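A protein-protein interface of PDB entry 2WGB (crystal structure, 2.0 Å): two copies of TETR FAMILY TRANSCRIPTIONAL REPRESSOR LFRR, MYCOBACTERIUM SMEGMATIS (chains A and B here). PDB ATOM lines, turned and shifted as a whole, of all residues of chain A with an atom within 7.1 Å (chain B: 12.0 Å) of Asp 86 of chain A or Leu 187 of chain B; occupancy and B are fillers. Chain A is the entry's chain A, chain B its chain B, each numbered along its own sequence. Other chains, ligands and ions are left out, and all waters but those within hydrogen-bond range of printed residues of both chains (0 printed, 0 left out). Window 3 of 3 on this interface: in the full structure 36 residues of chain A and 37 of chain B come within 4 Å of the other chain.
Among the printed residues, merely in contact across the chains: Asp 86 of chain A with Leu 187 of chain B (3.97 Å), Leu 89 of chain A with Ile 185 of chain B (3.1 Å) and Ala 136 of chain A with Ile 185 of chain B (3.4 Å).
No position is printed for both chains.
Of the 6 pairs that touch across the chains among the printed residues, none has its exchanged pair printed and touching as well.
Hydrophobic or aromatic side chains of chain B that line the printed part of chain A: Ile 185.
Of the 14 printed residues of chain A, 4 touch a printed residue of chain B.
Hydrophobic or aromatic side chains of chain A that line the printed part of chain B: Leu 89.
Among the printed residues, no Asp or Glu carboxylate lies within 4 Å of a Lys or Arg side-chain nitrogen of the other chain.
O of Met 177 of chain A lies within hydrogen-bond range of OG1 of Thr 181 of chain A.
Asp 86 of chain A touches just one residue of chain B: Leu 187.
Of chain A, only Asp 86 (3.97 Å) comes within 4 Å of Leu 187 of chain B.
Pro 84 of chain A touches none of the printed residues of chain B.
No residue of chain B comes within 4 Å of Val 85 of chain A.
Ala 88 of chain A touches none of the printed residues of chain B.
Leu 89 of chain A touches just one residue of chain B: Ile 185.
Ala 136 of chain A touches just these residues of chain B: Ile 185 (3.4 Å) and Thr 186 (3.1 Å).
Of the printed residues of chain A, Ile 185 of chain B touches Leu 89, Ala 136 and Thr 181.
Printed residues of chain A within 4 Å of Thr 186 of chain B: Ala 136.
Of the printed residues of chain A, Ser 182 of chain B touches Thr 181.
Arg 90 of chain A touches none of the printed residues of chain B.
Met 177 of chain A touches none of the printed residues of chain B.
The nearest residue of chain B that does not touch Asp 86 of chain A is Thr 186 of chain B (6.8 Å).
The nearest residue of chain A that does not touch Leu 187 of chain B is Thr 181 of chain A (4.2 Å).
O of Ala 136 of chain A sits at hydrogen-bond distance from N of Thr 186 of chain B.
O of Ile 185 of chain B sits close to O of Thr 181 of chain A (3.5 Å).
The backbone carbonyl oxygen of Ser 182 of chain B lies close to the backbone carbonyl oxygen of Thr 181 of chain A (3.4 Å).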
ATOM      1  N   GLY A  83      12.858 -11.261   8.810  1.00  0.00           N
ATOM      2  CA  GLY A  83      12.804 -10.213   7.813  1.00  0.00           C
ATOM      3  C   GLY A  83      13.640  -8.994   8.149  1.00  0.00           C
ATOM      4  O   GLY A  83      14.300  -8.951   9.192  1.00  0.00           O
ATOM      5  N   PRO A  84      13.602  -7.987   7.265  1.00  0.00           N
ATOM      6  CA  PRO A  84      14.375  -6.751   7.403  1.00  0.00           C
ATOM      7  C   PRO A  84      14.238  -6.200   8.804  1.00  0.00           C
ATOM      8  O   PRO A  84      13.128  -6.137   9.348  1.00  0.00           O
ATOM      9  CB  PRO A  84      13.704  -5.811   6.401  1.00  0.00           C
ATOM     10  CG  PRO A  84      13.167  -6.721   5.361  1.00  0.00           C
ATOM     11  CD  PRO A  84      12.708  -7.945   6.093  1.00  0.00           C
ATOM     12  N   VAL A  85      15.357  -5.804   9.394  1.00  0.00           N
ATOM     13  CA  VAL A  85      15.343  -5.399  10.789  1.00  0.00           C
ATOM     14  C   VAL A  85      14.546  -4.111  10.997  1.00  0.00           C
ATOM     15  O   VAL A  85      13.967  -3.897  12.062  1.00  0.00           O
ATOM     16  CB  VAL A  85      16.778  -5.299  11.375  1.00  0.00           C
ATOM     17  CG1 VAL A  85      17.487  -4.057  10.862  1.00  0.00           C
ATOM     18  CG2 VAL A  85      16.726  -5.304  12.887  1.00  0.00           C
ATOM     19  N   ASP A  86      14.485  -3.266   9.973  1.00  0.00           N
ATOM     20  CA  ASP A  86      13.721  -2.023  10.094  1.00  0.00           C
ATOM     21  C   ASP A  86      12.222  -2.282  10.238  1.00  0.00           C
ATOM     22  O   ASP A  86      11.552  -1.678  11.082  1.00  0.00           O
ATOM     23  CB  ASP A  86      14.009  -1.058   8.932  1.00  0.00           C
ATOM     24  CG  ASP A  86      13.811  -1.693   7.556  1.00  0.00           C
ATOM     25  OD1 ASP A  86      13.267  -2.814   7.462  1.00  0.00           O
ATOM     26  OD2 ASP A  86      14.204  -1.054   6.555  1.00  0.00           O
ATOM     27  N   ALA A  87      11.700  -3.192   9.424  1.00  0.00           N
ATOM     28  CA  ALA A  87      10.287  -3.543   9.483  1.00  0.00           C
ATOM     29  C   ALA A  87       9.970  -4.297  10.767  1.00  0.00           C
ATOM     30  O   ALA A  87       8.925  -4.077  11.386  1.00  0.00           O
ATOM     31  CB  ALA A  87       9.892  -4.375   8.251  1.00  0.00           C
ATOM     32  N   ALA A  88      10.873  -5.189  11.168  1.00  0.00           N
ATOM     33  CA  ALA A  88      10.692  -5.957  12.399  1.00  0.00           C
ATOM     34  C   ALA A  88      10.641  -5.045  13.642  1.00  0.00           C
ATOM     35  O   ALA A  88       9.793  -5.205  14.525  1.00  0.00           O
ATOM     36  CB  ALA A  88      11.797  -7.003  12.528  1.00  0.00           C
ATOM     37  N   LEU A  89      11.541  -4.074  13.701  1.00  0.00           N
ATOM     38  CA  LEU A  89      11.530  -3.122  14.808  1.00  0.00           C
ATOM     39  C   LEU A  89      10.212  -2.339  14.874  1.00  0.00           C
ATOM     40  O   LEU A  89       9.675  -2.105  15.957  1.00  0.00           O
ATOM     41  CB  LEU A  89      12.715  -2.163  14.693  1.00  0.00           C
ATOM     42  CG  LEU A  89      12.915  -1.220  15.878  1.00  0.00           C
ATOM     43  CD1 LEU A  89      13.083  -2.001  17.189  1.00  0.00           C
ATOM     44  CD2 LEU A  89      14.130  -0.367  15.609  1.00  0.00           C
ATOM     45  N   ARG A  90       9.696  -1.919  13.722  1.00  0.00           N
ATOM     46  CA  ARG A  90       8.432  -1.194  13.693  1.00  0.00           C
ATOM     47  C   ARG A  90       7.276  -2.038  14.226  1.00  0.00           C
ATOM     48  O   ARG A  90       6.438  -1.551  14.974  1.00  0.00           O
ATOM     49  CB  ARG A  90       8.098  -0.685  12.286  1.00  0.00           C
ATOM     50  CG  ARG A  90       6.717  -0.044  12.228  1.00  0.00           C
ATOM     51  CD  ARG A  90       6.370   0.542  10.864  1.00  0.00           C
ATOM     52  NE  ARG A  90       5.210   1.423  10.976  1.00  0.00           N
ATOM     53  CZ  ARG A  90       5.285   2.747  11.052  1.00  0.00           C
ATOM     54  NH1 ARG A  90       6.465   3.344  11.010  1.00  0.00           N
ATOM     55  NH2 ARG A  90       4.181   3.473  11.164  1.00  0.00           N
ATOM     56  N   ARG A  91       7.224  -3.307  13.828  1.00  0.00           N
ATOM     57  CA  ARG A  91       6.217  -4.224  14.362  1.00  0.00           C
ATOM     58  C   ARG A  91       6.340  -4.357  15.885  1.00  0.00           C
ATOM     59  O   ARG A  91       5.340  -4.394  16.591  1.00  0.00           O
ATOM     60  CB  ARG A  91       6.321  -5.618  13.713  1.00  0.00           C
ATOM     61  CG  ARG A  91       5.993  -5.657  12.225  1.00  0.00           C
ATOM     62  CD  ARG A  91       5.710  -7.083  11.743  1.00  0.00           C
ATOM     63  NE  ARG A  91       6.838  -7.968  11.995  1.00  0.00           N
ATOM     64  CZ  ARG A  91       7.854  -8.154  11.161  1.00  0.00           C
ATOM     65  NH1 ARG A  91       7.894  -7.527   9.996  1.00  0.00           N
ATOM     66  NH2 ARG A  91       8.829  -8.973  11.494  1.00  0.00           N
ATOM     67  N   VAL A 132      16.338  -8.179  18.681  1.00  0.00           N
ATOM     68  CA  VAL A 132      16.082  -7.329  17.516  1.00  0.00           C
ATOM     69  C   VAL A 132      16.919  -6.053  17.568  1.00  0.00           C
ATOM     70  O   VAL A 132      17.449  -5.615  16.545  1.00  0.00           O
ATOM     71  CB  VAL A 132      14.569  -7.016  17.294  1.00  0.00           C
ATOM     72  CG1 VAL A 132      14.031  -6.081  18.362  1.00  0.00           C
ATOM     73  CG2 VAL A 132      14.354  -6.405  15.909  1.00  0.00           C
ATOM     74  N   ARG A 135      20.349  -6.898  16.507  1.00  0.00           N
ATOM     75  CA  ARG A 135      20.373  -7.106  15.063  1.00  0.00           C
ATOM     76  C   ARG A 135      20.551  -5.757  14.347  1.00  0.00           C
ATOM     77  O   ARG A 135      21.092  -5.692  13.249  1.00  0.00           O
ATOM     78  CB  ARG A 135      19.070  -7.803  14.634  1.00  0.00           C
ATOM     79  CG  ARG A 135      19.067  -8.405  13.239  1.00  0.00           C
ATOM     80  CD  ARG A 135      18.238  -9.697  13.181  1.00  0.00           C
ATOM     81  NE  ARG A 135      16.787  -9.486  13.183  1.00  0.00           N
ATOM     82  CZ  ARG A 135      16.058  -9.302  12.081  1.00  0.00           C
ATOM     83  NH1 ARG A 135      14.744  -9.128  12.165  1.00  0.00           N
ATOM     84  NH2 ARG A 135      16.644  -9.287  10.893  1.00  0.00           N
ATOM     85  N   ALA A 136      20.105  -4.680  14.992  1.00  0.00           N
ATOM     86  CA  ALA A 136      20.145  -3.339  14.402  1.00  0.00           C
ATOM     87  C   ALA A 136      21.247  -2.435  14.967  1.00  0.00           C
ATOM     88  O   ALA A 136      21.249  -1.229  14.725  1.00  0.00           O
ATOM     89  CB  ALA A 136      18.786  -2.663  14.568  1.00  0.00           C
ATOM     90  N   MET A 177      10.284   5.522  16.143  1.00  0.00           N
ATOM     91  CA  MET A 177      11.176   4.951  15.141  1.00  0.00           C
ATOM     92  C   MET A 177      12.286   5.935  14.715  1.00  0.00           C
ATOM     93  O   MET A 177      13.452   5.556  14.600  1.00  0.00           O
ATOM     94  CB  MET A 177      10.380   4.467  13.921  1.00  0.00           C
ATOM     95  CG  MET A 177       9.606   3.162  14.141  1.00  0.00           C
ATOM     96  SD  MET A 177      10.636   1.750  14.625  1.00  0.00           S
ATOM     97  CE  MET A 177      11.687   1.598  13.179  1.00  0.00           C
ATOM     98  N   THR A 181      16.441   5.775  15.440  1.00  0.00           N
ATOM     99  CA  THR A 181      17.421   5.683  14.351  1.00  0.00           C
ATOM    100  C   THR A 181      18.208   6.965  14.107  1.00  0.00           C
ATOM    101  O   THR A 181      19.294   6.922  13.531  1.00  0.00           O
ATOM    102  CB  THR A 181      16.773   5.241  13.014  1.00  0.00           C
ATOM    103  OG1 THR A 181      15.835   6.232  12.572  1.00  0.00           O
ATOM    104  CG2 THR A 181      16.055   3.914  13.177  1.00  0.00           C
ATOM    105  N   SER B 182      22.273  11.303  17.460  1.00  0.00           N
ATOM    106  CA  SER B 182      22.225  10.358  16.350  1.00  0.00           C
ATOM    107  C   SER B 182      21.418   9.084  16.570  1.00  0.00           C
ATOM    108  O   SER B 182      21.484   8.182  15.748  1.00  0.00           O
ATOM    109  CB  SER B 182      23.647   9.993  15.911  1.00  0.00           C
ATOM    110  OG  SER B 182      24.456   9.659  17.022  1.00  0.00           O
ATOM    111  N   GLY B 183      20.654   9.002  17.656  1.00  0.00           N
ATOM    112  CA  GLY B 183      19.890   7.793  17.931  1.00  0.00           C
ATOM    113  C   GLY B 183      20.767   6.643  18.404  1.00  0.00           C
ATOM    114  O   GLY B 183      21.973   6.812  18.587  1.00  0.00           O
ATOM    115  N   ILE B 184      20.175   5.467  18.594  1.00  0.00           N
ATOM    116  CA  ILE B 184      20.919   4.345  19.162  1.00  0.00           C
ATOM    117  C   ILE B 184      21.116   3.183  18.197  1.00  0.00           C
ATOM    118  O   ILE B 184      21.918   2.292  18.462  1.00  0.00           O
ATOM    119  CB  ILE B 184      20.281   3.807  20.476  1.00  0.00           C
ATOM    120  CG1 ILE B 184      18.816   3.439  20.245  1.00  0.00           C
ATOM    121  CG2 ILE B 184      20.438   4.833  21.607  1.00  0.00           C
ATOM    122  CD1 ILE B 184      18.275   2.379  21.206  1.00  0.00           C
ATOM    123  N   ILE B 185      20.388   3.186  17.082  1.00  0.00           N
ATOM    124  CA  ILE B 185      20.502   2.099  16.118  1.00  0.00           C
ATOM    125  C   ILE B 185      20.628   2.588  14.676  1.00  0.00           C
ATOM    126  O   ILE B 185      20.354   3.747  14.372  1.00  0.00           O
ATOM    127  CB  ILE B 185      19.306   1.139  16.206  1.00  0.00           C
ATOM    128  CG1 ILE B 185      18.034   1.850  15.767  1.00  0.00           C
ATOM    129  CG2 ILE B 185      19.160   0.581  17.619  1.00  0.00           C
ATOM    130  CD1 ILE B 185      16.795   1.119  16.167  1.00  0.00           C
ATOM    131  N   THR B 186      21.024   1.685  13.785  1.00  0.00           N
ATOM    132  CA  THR B 186      21.215   2.030  12.380  1.00  0.00           C
ATOM    133  C   THR B 186      20.321   1.194  11.472  1.00  0.00           C
ATOM    134  O   THR B 186      20.197  -0.015  11.658  1.00  0.00           O
ATOM    135  CB  THR B 186      22.678   1.839  11.964  1.00  0.00           C
ATOM    136  OG1 THR B 186      23.082   0.500  12.266  1.00  0.00           O
ATOM    137  CG2 THR B 186      23.577   2.818  12.713  1.00  0.00           C
ATOM    138  N   LEU B 187      19.706   1.855  10.492  1.00  0.00           N
ATOM    139  CA  LEU B 187      18.756   1.234   9.567  1.00  0.00           C
ATOM    140  C   LEU B 187      17.342   1.264  10.136  1.00  0.00           C
ATOM    141  O   LEU B 187      17.006   0.484  11.027  1.00  0.00           O
ATOM    142  CB  LEU B 187      19.155  -0.205   9.219  1.00  0.00           C
ATOM    143  CG  LEU B 187      20.443  -0.439   8.427  1.00  0.00           C
ATOM    144  CD1 LEU B 187      20.793  -1.921   8.405  1.00  0.00           C
ATOM    145  CD2 LEU B 187      20.315   0.106   7.012  1.00  0.00           C
